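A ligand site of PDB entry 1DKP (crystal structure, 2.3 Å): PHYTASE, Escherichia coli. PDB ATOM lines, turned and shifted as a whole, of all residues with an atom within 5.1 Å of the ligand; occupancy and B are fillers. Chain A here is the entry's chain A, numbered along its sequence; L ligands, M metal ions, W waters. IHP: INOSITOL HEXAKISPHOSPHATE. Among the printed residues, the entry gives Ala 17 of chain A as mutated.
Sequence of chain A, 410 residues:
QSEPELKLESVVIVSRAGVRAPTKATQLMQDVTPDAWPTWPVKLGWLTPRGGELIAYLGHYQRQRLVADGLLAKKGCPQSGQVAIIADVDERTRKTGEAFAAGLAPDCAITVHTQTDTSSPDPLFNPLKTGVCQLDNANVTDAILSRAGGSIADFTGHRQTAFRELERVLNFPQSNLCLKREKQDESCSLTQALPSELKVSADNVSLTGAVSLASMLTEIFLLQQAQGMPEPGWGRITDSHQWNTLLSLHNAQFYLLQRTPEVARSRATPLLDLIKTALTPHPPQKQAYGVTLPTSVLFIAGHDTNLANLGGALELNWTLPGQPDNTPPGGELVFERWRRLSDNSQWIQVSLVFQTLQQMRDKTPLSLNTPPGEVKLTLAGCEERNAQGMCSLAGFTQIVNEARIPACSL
NE of Arg 92 lies within salt-bridge range of O33 of the ligand. The guanidinium group (NE) of Arg 16 lies within salt-bridge range of an oxygen (O43) of the ligand (2.8 Å). An oxygen (O22) of the ligand is in salt-bridge range of the guanidinium group (NH2) of Arg 267, at 3.1 Å. An oxygen (O24) of the ligand lies close to the side-chain carboxylate of Asp 304, 2.5 Å away. OG1 of Thr 305 is in hydrogen-bond range of O42 of the ligand, 2.5 Å away. NZ of Lys 24 lies within salt-bridge range of O26 of the ligand (2.9 Å). ND1 of His 303 lies within hydrogen-bond range of O33 of the ligand (2.6 Å). An oxygen (O43) of the ligand is in hydrogen-bond range of the backbone NH (N) of Asp 304. An oxygen (O23) of the ligand is in salt-bridge range of the guanidinium group (NE) of Arg 20, at 2.8 Å. OG1 of Thr 23 sits at hydrogen-bond distance from O25 of the ligand (2.6 Å).
ND1 of His 250 sits at hydrogen-bond distance from O of Ser 215 (2.7 Å). A ring nitrogen (NE2) of His 303 sits close to the side-chain carboxylate of Asp 90. NE2 of His 250 sits at hydrogen-bond distance from OE2 of Glu 219 (3.4 Å). OD1 of Asn 306 sits at hydrogen-bond distance from N of His 303 (2.6 Å). The side-chain carboxylate (OE1) of Glu 219 lies within salt-bridge range of the guanidinium group (NH2) of Arg 16, 3.0 Å away. The side-chain hydroxyl (OG1) of Thr 305 is in hydrogen-bond range of the guanidinium group (NH1) of Arg 267. OD1 of Asp 304 lies within salt-bridge range of NH2 of Arg 16, at 3.5 Å.
Merely in contact with the ligand: Asp 90, Met 216, Glu 219, His 250 and Phe 254. 14 residues have an atom within 4 Å of the ligand: Arg 16, Arg 20, Thr 23, Lys 24, Asp 90, Arg 92, Met 216, Glu 219, His 250, Phe 254, Arg 267, His 303, Asp 304 and Thr 305. Along chain A the residues within 4 Å of the ligand span positions 16 to 305.
Water W1 lies within hydrogen-bond range of OD2 of Asp 90 (2.5 Å), O41 of the ligand (2.7 Å) and NE2 of His 303 (2.7 Å). Water W2 lies within hydrogen-bond range of O25 of the ligand (2.7 Å), N of Thr 23 (3.0 Å) and NH2 of Arg 20 (3.3 Å). Water W5 lies within hydrogen-bond range of an oxygen (O23) of the ligand (2.7 Å) and the guanidinium group (NE) of Arg 20 (3.1 Å). Water W6 bridges an oxygen (O44) of the ligand (2.8 Å) and the guanidinium group of Arg 20 (3.4 Å). Water W7 bridges the side-chain hydroxyl of Ser 215 (2.7 Å) and an oxygen (O44) of the ligand (3.0 Å).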
ATOM      1  N   ARG A  16      12.705 -21.991 -17.583  1.00  0.00           N
ATOM      2  CA  ARG A  16      13.637 -22.521 -16.622  1.00  0.00           C
ATOM      3  C   ARG A  16      12.733 -23.221 -15.620  1.00  0.00           C
ATOM      4  O   ARG A  16      11.552 -22.882 -15.518  1.00  0.00           O
ATOM      5  CB  ARG A  16      14.383 -21.400 -15.907  1.00  0.00           C
ATOM      6  CG  ARG A  16      15.251 -21.946 -14.783  1.00  0.00           C
ATOM      7  CD  ARG A  16      16.014 -20.875 -14.037  1.00  0.00           C
ATOM      8  NE  ARG A  16      16.822 -21.515 -13.003  1.00  0.00           N
ATOM      9  CZ  ARG A  16      17.248 -20.921 -11.896  1.00  0.00           C
ATOM     10  NH1 ARG A  16      16.932 -19.655 -11.662  1.00  0.00           N
ATOM     11  NH2 ARG A  16      17.961 -21.602 -11.012  1.00  0.00           N
ATOM     12  N   ALA A  17      13.274 -24.187 -14.890  1.00  0.00           N
ATOM     13  CA  ALA A  17      12.487 -24.891 -13.888  1.00  0.00           C
ATOM     14  C   ALA A  17      12.090 -23.872 -12.816  1.00  0.00           C
ATOM     15  O   ALA A  17      12.672 -22.785 -12.715  1.00  0.00           O
ATOM     16  CB  ALA A  17      13.301 -26.015 -13.271  1.00  0.00           C
ATOM     17  N   ARG A  20      13.190 -24.387  -6.486  1.00  0.00           N
ATOM     18  CA  ARG A  20      13.649 -25.700  -6.041  1.00  0.00           C
ATOM     19  C   ARG A  20      14.603 -25.560  -4.851  1.00  0.00           C
ATOM     20  O   ARG A  20      15.090 -24.465  -4.555  1.00  0.00           O
ATOM     21  CB  ARG A  20      14.401 -26.392  -7.187  1.00  0.00           C
ATOM     22  CG  ARG A  20      15.630 -25.567  -7.634  1.00  0.00           C
ATOM     23  CD  ARG A  20      16.614 -26.358  -8.496  1.00  0.00           C
ATOM     24  NE  ARG A  20      17.687 -25.511  -9.019  1.00  0.00           N
ATOM     25  CZ  ARG A  20      18.680 -24.991  -8.280  1.00  0.00           C
ATOM     26  NH1 ARG A  20      19.604 -24.229  -8.854  1.00  0.00           N
ATOM     27  NH2 ARG A  20      18.751 -25.238  -6.979  1.00  0.00           N
ATOM     28  N   THR A  23      20.804 -27.502  -5.068  1.00  0.00           N
ATOM     29  CA  THR A  23      21.207 -28.813  -5.597  1.00  0.00           C
ATOM     30  C   THR A  23      22.235 -29.555  -4.747  1.00  0.00           C
ATOM     31  O   THR A  23      22.382 -30.769  -4.878  1.00  0.00           O
ATOM     32  CB  THR A  23      21.782 -28.705  -7.026  1.00  0.00           C
ATOM     33  OG1 THR A  23      22.937 -27.861  -7.007  1.00  0.00           O
ATOM     34  CG2 THR A  23      20.739 -28.138  -7.987  1.00  0.00           C
ATOM     35  N   LYS A  24      22.948 -28.836  -3.883  1.00  0.00           N
ATOM     36  CA  LYS A  24      23.939 -29.491  -3.045  1.00  0.00           C
ATOM     37  C   LYS A  24      24.082 -28.856  -1.673  1.00  0.00           C
ATOM     38  O   LYS A  24      23.614 -27.749  -1.428  1.00  0.00           O
ATOM     39  CB  LYS A  24      25.293 -29.530  -3.748  1.00  0.00           C
ATOM     40  CG  LYS A  24      25.818 -28.176  -4.184  1.00  0.00           C
ATOM     41  CD  LYS A  24      26.959 -28.328  -5.176  1.00  0.00           C
ATOM     42  CE  LYS A  24      26.498 -29.023  -6.454  1.00  0.00           C
ATOM     43  NZ  LYS A  24      27.590 -29.175  -7.460  1.00  0.00           N
ATOM     44  N   ASP A  90      15.259 -34.239 -15.685  1.00  0.00           N
ATOM     45  CA  ASP A  90      15.346 -33.913 -14.261  1.00  0.00           C
ATOM     46  C   ASP A  90      13.959 -33.874 -13.609  1.00  0.00           C
ATOM     47  O   ASP A  90      12.965 -33.546 -14.256  1.00  0.00           O
ATOM     48  CB  ASP A  90      16.044 -32.555 -14.062  1.00  0.00           C
ATOM     49  CG  ASP A  90      17.478 -32.546 -14.581  1.00  0.00           C
ATOM     50  OD1 ASP A  90      18.200 -33.562 -14.389  1.00  0.00           O
ATOM     51  OD2 ASP A  90      17.898 -31.536 -15.174  1.00  0.00           O
ATOM     52  N   ARG A  92      12.861 -31.787 -11.426  1.00  0.00           N
ATOM     53  CA  ARG A  92      12.344 -30.430 -11.384  1.00  0.00           C
ATOM     54  C   ARG A  92      11.797 -29.925 -12.713  1.00  0.00           C
ATOM     55  O   ARG A  92      10.845 -29.149 -12.735  1.00  0.00           O
ATOM     56  CB  ARG A  92      13.399 -29.455 -10.837  1.00  0.00           C
ATOM     57  CG  ARG A  92      14.708 -29.368 -11.602  1.00  0.00           C
ATOM     58  CD  ARG A  92      15.530 -28.214 -11.024  1.00  0.00           C
ATOM     59  NE  ARG A  92      16.842 -28.057 -11.639  1.00  0.00           N
ATOM     60  CZ  ARG A  92      17.864 -28.899 -11.470  1.00  0.00           C
ATOM     61  NH1 ARG A  92      17.729 -29.977 -10.701  1.00  0.00           N
ATOM     62  NH2 ARG A  92      19.020 -28.663 -12.071  1.00  0.00           N
ATOM     63  N   LYS A 129      27.924 -32.141 -22.748  1.00  0.00           N
ATOM     64  CA  LYS A 129      28.033 -33.146 -21.707  1.00  0.00           C
ATOM     65  C   LYS A 129      27.784 -34.567 -22.201  1.00  0.00           C
ATOM     66  O   LYS A 129      28.364 -35.521 -21.690  1.00  0.00           O
ATOM     67  CB  LYS A 129      27.048 -32.803 -20.585  1.00  0.00           C
ATOM     68  CG  LYS A 129      27.130 -33.664 -19.346  1.00  0.00           C
ATOM     69  CD  LYS A 129      26.204 -33.124 -18.248  1.00  0.00           C
ATOM     70  CE  LYS A 129      24.757 -33.063 -18.719  1.00  0.00           C
ATOM     71  NZ  LYS A 129      23.862 -32.477 -17.677  1.00  0.00           N
ATOM     72  N   SER A 215      28.208 -17.500  -6.859  1.00  0.00           N
ATOM     73  CA  SER A 215      27.091 -17.614  -7.809  1.00  0.00           C
ATOM     74  C   SER A 215      26.036 -18.581  -7.293  1.00  0.00           C
ATOM     75  O   SER A 215      24.845 -18.359  -7.490  1.00  0.00           O
ATOM     76  CB  SER A 215      27.587 -18.096  -9.174  1.00  0.00           C
ATOM     77  OG  SER A 215      26.484 -18.296 -10.046  1.00  0.00           O
ATOM     78  N   MET A 216      26.459 -19.656  -6.647  1.00  0.00           N
ATOM     79  CA  MET A 216      25.514 -20.639  -6.110  1.00  0.00           C
ATOM     80  C   MET A 216      24.836 -20.114  -4.842  1.00  0.00           C
ATOM     81  O   MET A 216      23.617 -20.206  -4.694  1.00  0.00           O
ATOM     82  CB  MET A 216      26.246 -21.935  -5.794  1.00  0.00           C
ATOM     83  CG  MET A 216      25.333 -23.071  -5.356  1.00  0.00           C
ATOM     84  SD  MET A 216      26.242 -24.404  -4.564  1.00  0.00           S
ATOM     85  CE  MET A 216      27.400 -24.830  -5.838  1.00  0.00           C
ATOM     86  N   GLU A 219      22.188 -17.457  -5.438  1.00  0.00           N
ATOM     87  CA  GLU A 219      21.004 -18.034  -6.053  1.00  0.00           C
ATOM     88  C   GLU A 219      20.174 -18.694  -4.950  1.00  0.00           C
ATOM     89  O   GLU A 219      18.942 -18.619  -4.956  1.00  0.00           O
ATOM     90  CB  GLU A 219      21.385 -19.075  -7.108  1.00  0.00           C
ATOM     91  CG  GLU A 219      20.203 -19.861  -7.654  1.00  0.00           C
ATOM     92  CD  GLU A 219      19.255 -19.017  -8.491  1.00  0.00           C
ATOM     93  OE1 GLU A 219      18.159 -19.529  -8.843  1.00  0.00           O
ATOM     94  OE2 GLU A 219      19.594 -17.860  -8.810  1.00  0.00           O
ATOM     95  N   HIS A 250      25.915 -13.794  -9.359  1.00  0.00           N
ATOM     96  CA  HIS A 250      25.324 -14.916 -10.061  1.00  0.00           C
ATOM     97  C   HIS A 250      25.290 -14.614 -11.561  1.00  0.00           C
ATOM     98  O   HIS A 250      25.767 -15.389 -12.379  1.00  0.00           O
ATOM     99  CB  HIS A 250      23.920 -15.150  -9.517  1.00  0.00           C
ATOM    100  CG  HIS A 250      23.246 -16.342 -10.097  1.00  0.00           C
ATOM    101  ND1 HIS A 250      23.644 -17.630  -9.812  1.00  0.00           N
ATOM    102  CD2 HIS A 250      22.226 -16.445 -10.970  1.00  0.00           C
ATOM    103  CE1 HIS A 250      22.895 -18.478 -10.492  1.00  0.00           C
ATOM    104  NE2 HIS A 250      22.034 -17.782 -11.206  1.00  0.00           N
ATOM    105  N   PHE A 254      27.307 -16.349 -15.126  1.00  0.00           N
ATOM    106  CA  PHE A 254      26.612 -16.741 -16.343  1.00  0.00           C
ATOM    107  C   PHE A 254      27.081 -15.933 -17.542  1.00  0.00           C
ATOM    108  O   PHE A 254      27.120 -16.439 -18.667  1.00  0.00           O
ATOM    109  CB  PHE A 254      25.099 -16.617 -16.149  1.00  0.00           C
ATOM    110  CG  PHE A 254      24.478 -17.822 -15.503  1.00  0.00           C
ATOM    111  CD1 PHE A 254      24.841 -18.186 -14.198  1.00  0.00           C
ATOM    112  CD2 PHE A 254      23.579 -18.623 -16.192  1.00  0.00           C
ATOM    113  CE1 PHE A 254      24.309 -19.331 -13.614  1.00  0.00           C
ATOM    114  CE2 PHE A 254      23.030 -19.774 -15.607  1.00  0.00           C
ATOM    115  CZ  PHE A 254      23.406 -20.125 -14.314  1.00  0.00           C
ATOM    116  N   ARG A 267      26.291 -25.077 -27.150  1.00  0.00           N
ATOM    117  CA  ARG A 267      25.345 -25.552 -26.129  1.00  0.00           C
ATOM    118  C   ARG A 267      23.875 -25.274 -26.442  1.00  0.00           C
ATOM    119  O   ARG A 267      22.990 -25.977 -25.943  1.00  0.00           O
ATOM    120  CB  ARG A 267      25.698 -24.925 -24.773  1.00  0.00           C
ATOM    121  CG  ARG A 267      25.248 -25.715 -23.541  1.00  0.00           C
ATOM    122  CD  ARG A 267      26.098 -25.329 -22.325  1.00  0.00           C
ATOM    123  NE  ARG A 267      25.766 -26.075 -21.112  1.00  0.00           N
ATOM    124  CZ  ARG A 267      24.618 -25.948 -20.437  1.00  0.00           C
ATOM    125  NH1 ARG A 267      23.688 -25.087 -20.852  1.00  0.00           N
ATOM    126  NH2 ARG A 267      24.400 -26.694 -19.358  1.00  0.00           N
ATOM    127  N   GLY A 302      13.375 -26.286 -19.391  1.00  0.00           N
ATOM    128  CA  GLY A 302      14.818 -26.436 -19.341  1.00  0.00           C
ATOM    129  C   GLY A 302      15.445 -25.813 -18.111  1.00  0.00           C
ATOM    130  O   GLY A 302      14.866 -25.829 -17.019  1.00  0.00           O
ATOM    131  N   HIS A 303      16.615 -25.200 -18.292  1.00  0.00           N
ATOM    132  CA  HIS A 303      17.358 -24.622 -17.190  1.00  0.00           C
ATOM    133  C   HIS A 303      17.795 -23.181 -17.451  1.00  0.00           C
ATOM    134  O   HIS A 303      17.601 -22.637 -18.533  1.00  0.00           O
ATOM    135  CB  HIS A 303      18.596 -25.481 -16.915  1.00  0.00           C
ATOM    136  CG  HIS A 303      18.304 -26.946 -16.821  1.00  0.00           C
ATOM    137  ND1 HIS A 303      17.910 -27.553 -15.647  1.00  0.00           N
ATOM    138  CD2 HIS A 303      18.336 -27.925 -17.754  1.00  0.00           C
ATOM    139  CE1 HIS A 303      17.729 -28.850 -15.860  1.00  0.00           C
ATOM    140  NE2 HIS A 303      17.981 -29.103 -17.132  1.00  0.00           N
ATOM    141  N   ASP A 304      18.401 -22.567 -16.429  1.00  0.00           N
ATOM    142  CA  ASP A 304      18.856 -21.205 -16.590  1.00  0.00           C
ATOM    143  C   ASP A 304      19.983 -21.125 -17.608  1.00  0.00           C
ATOM    144  O   ASP A 304      20.062 -20.165 -18.380  1.00  0.00           O
ATOM    145  CB  ASP A 304      19.276 -20.613 -15.240  1.00  0.00           C
ATOM    146  CG  ASP A 304      20.231 -21.500 -14.476  1.00  0.00           C
ATOM    147  OD1 ASP A 304      20.512 -21.171 -13.308  1.00  0.00           O
ATOM    148  OD2 ASP A 304      20.698 -22.507 -15.038  1.00  0.00           O
ATOM    149  N   THR A 305      20.840 -22.140 -17.641  1.00  0.00           N
ATOM    150  CA  THR A 305      21.944 -22.111 -18.608  1.00  0.00           C
ATOM    151  C   THR A 305      21.416 -22.107 -20.048  1.00  0.00           C
ATOM    152  O   THR A 305      22.041 -21.545 -20.947  1.00  0.00           O
ATOM    153  CB  THR A 305      22.879 -23.301 -18.421  1.00  0.00           C
ATOM    154  OG1 THR A 305      22.161 -24.518 -18.678  1.00  0.00           O
ATOM    155  CG2 THR A 305      23.453 -23.300 -17.016  1.00  0.00           C
ATOM    156  N   ASN A 306      20.260 -22.736 -20.262  1.00  0.00           N
ATOM    157  CA  ASN A 306      19.651 -22.787 -21.595  1.00  0.00           C
ATOM    158  C   ASN A 306      19.213 -21.393 -22.018  1.00  0.00           C
ATOM    159  O   ASN A 306      19.464 -20.969 -23.145  1.00  0.00           O
ATOM    160  CB  ASN A 306      18.437 -23.722 -21.581  1.00  0.00           C
ATOM    161  CG  ASN A 306      18.791 -25.142 -21.181  1.00  0.00           C
ATOM    162  OD1 ASN A 306      18.152 -25.735 -20.316  1.00  0.00           O
ATOM    163  ND2 ASN A 306      19.834 -25.702 -21.810  1.00  0.00           N
HETATM  164  C1  IHP L   1      22.466 -27.921 -12.171  1.00  0.00           C
HETATM  165  C2  IHP L   1      21.626 -26.935 -13.072  1.00  0.00           C
HETATM  166  C3  IHP L   1      21.049 -25.732 -12.223  1.00  0.00           C
HETATM  167  C4  IHP L   1      22.228 -24.941 -11.501  1.00  0.00           C
HETATM  168  C5  IHP L   1      23.171 -25.917 -10.715  1.00  0.00           C
HETATM  169  C6  IHP L   1      23.645 -27.119 -11.563  1.00  0.00           C
HETATM  170  O11 IHP L   1      22.991 -29.005 -12.963  1.00  0.00           O
HETATM  171  P1  IHP L   1      22.109 -30.302 -13.299  1.00  0.00           P
HETATM  172  O21 IHP L   1      21.266 -30.701 -12.002  1.00  0.00           O
HETATM  173  O31 IHP L   1      23.029 -31.418 -13.676  1.00  0.00           O
HETATM  174  O41 IHP L   1      21.091 -30.049 -14.492  1.00  0.00           O
HETATM  175  O12 IHP L   1      22.454 -26.386 -14.118  1.00  0.00           O
HETATM  176  P2  IHP L   1      22.228 -26.709 -15.678  1.00  0.00           P
HETATM  177  O22 IHP L   1      23.604 -27.124 -16.376  1.00  0.00           O
HETATM  178  O32 IHP L   1      21.239 -27.815 -15.879  1.00  0.00           O
HETATM  179  O42 IHP L   1      21.676 -25.414 -16.414  1.00  0.00           O
HETATM  180  O13 IHP L   1      20.298 -24.856 -13.072  1.00  0.00           O
HETATM  181  P3  IHP L   1      18.673 -24.894 -13.009  1.00  0.00           P
HETATM  182  O23 IHP L   1      18.194 -24.564 -11.644  1.00  0.00           O
HETATM  183  O33 IHP L   1      18.145 -26.331 -13.408  1.00  0.00           O
HETATM  184  O43 IHP L   1      18.098 -23.834 -14.041  1.00  0.00           O
HETATM  185  O14 IHP L   1      21.715 -23.986 -10.572  1.00  0.00           O
HETATM  186  P4  IHP L   1      22.206 -22.444 -10.675  1.00  0.00           P
HETATM  187  O24 IHP L   1      21.001 -21.588 -10.874  1.00  0.00           O
HETATM  188  O34 IHP L   1      23.239 -22.177 -11.866  1.00  0.00           O
HETATM  189  O44 IHP L   1      22.885 -22.028  -9.300  1.00  0.00           O
HETATM  190  O15 IHP L   1      24.350 -25.246 -10.236  1.00  0.00           O
HETATM  191  P5  IHP L   1      24.619 -25.045  -8.663  1.00  0.00           P
HETATM  192  O25 IHP L   1      23.436 -25.469  -7.851  1.00  0.00           O
HETATM  193  O35 IHP L   1      25.906 -25.878  -8.254  1.00  0.00           O
HETATM  194  O45 IHP L   1      24.880 -23.500  -8.385  1.00  0.00           O
HETATM  195  O16 IHP L   1      24.456 -27.959 -10.714  1.00  0.00           O
HETATM  196  P6  IHP L   1      25.993 -28.231 -11.064  1.00  0.00           P
HETATM  197  O26 IHP L   1      26.506 -29.456 -10.185  1.00  0.00           O
HETATM  198  O36 IHP L   1      26.862 -26.949 -10.716  1.00  0.00           O
HETATM  199  O46 IHP L   1      26.140 -28.564 -12.510  1.00  0.00           O
HETATM  200 HG    HG M   1      19.656 -18.799 -11.649  1.00  0.00          HG
HETATM  201 HG    HG M   2      20.004 -17.918 -13.020  1.00  0.00          HG
HETATM  202  O   HOH W   1      19.857 -31.020 -16.698  1.00  0.00           O
HETATM  203  O   HOH W   2      21.806 -24.741  -5.814  1.00  0.00           O
HETATM  204  O   HOH W   3      25.352 -23.338 -13.602  1.00  0.00           O
HETATM  205  O   HOH W   4      21.268 -28.728 -18.935  1.00  0.00           O
HETATM  206  O   HOH W   5      15.508 -24.734 -11.092  1.00  0.00           O
HETATM  207  O   HOH W   6      21.779 -22.533  -6.792  1.00  0.00           O
HETATM  208  O   HOH W   7      25.504 -20.861 -10.060  1.00  0.00           O
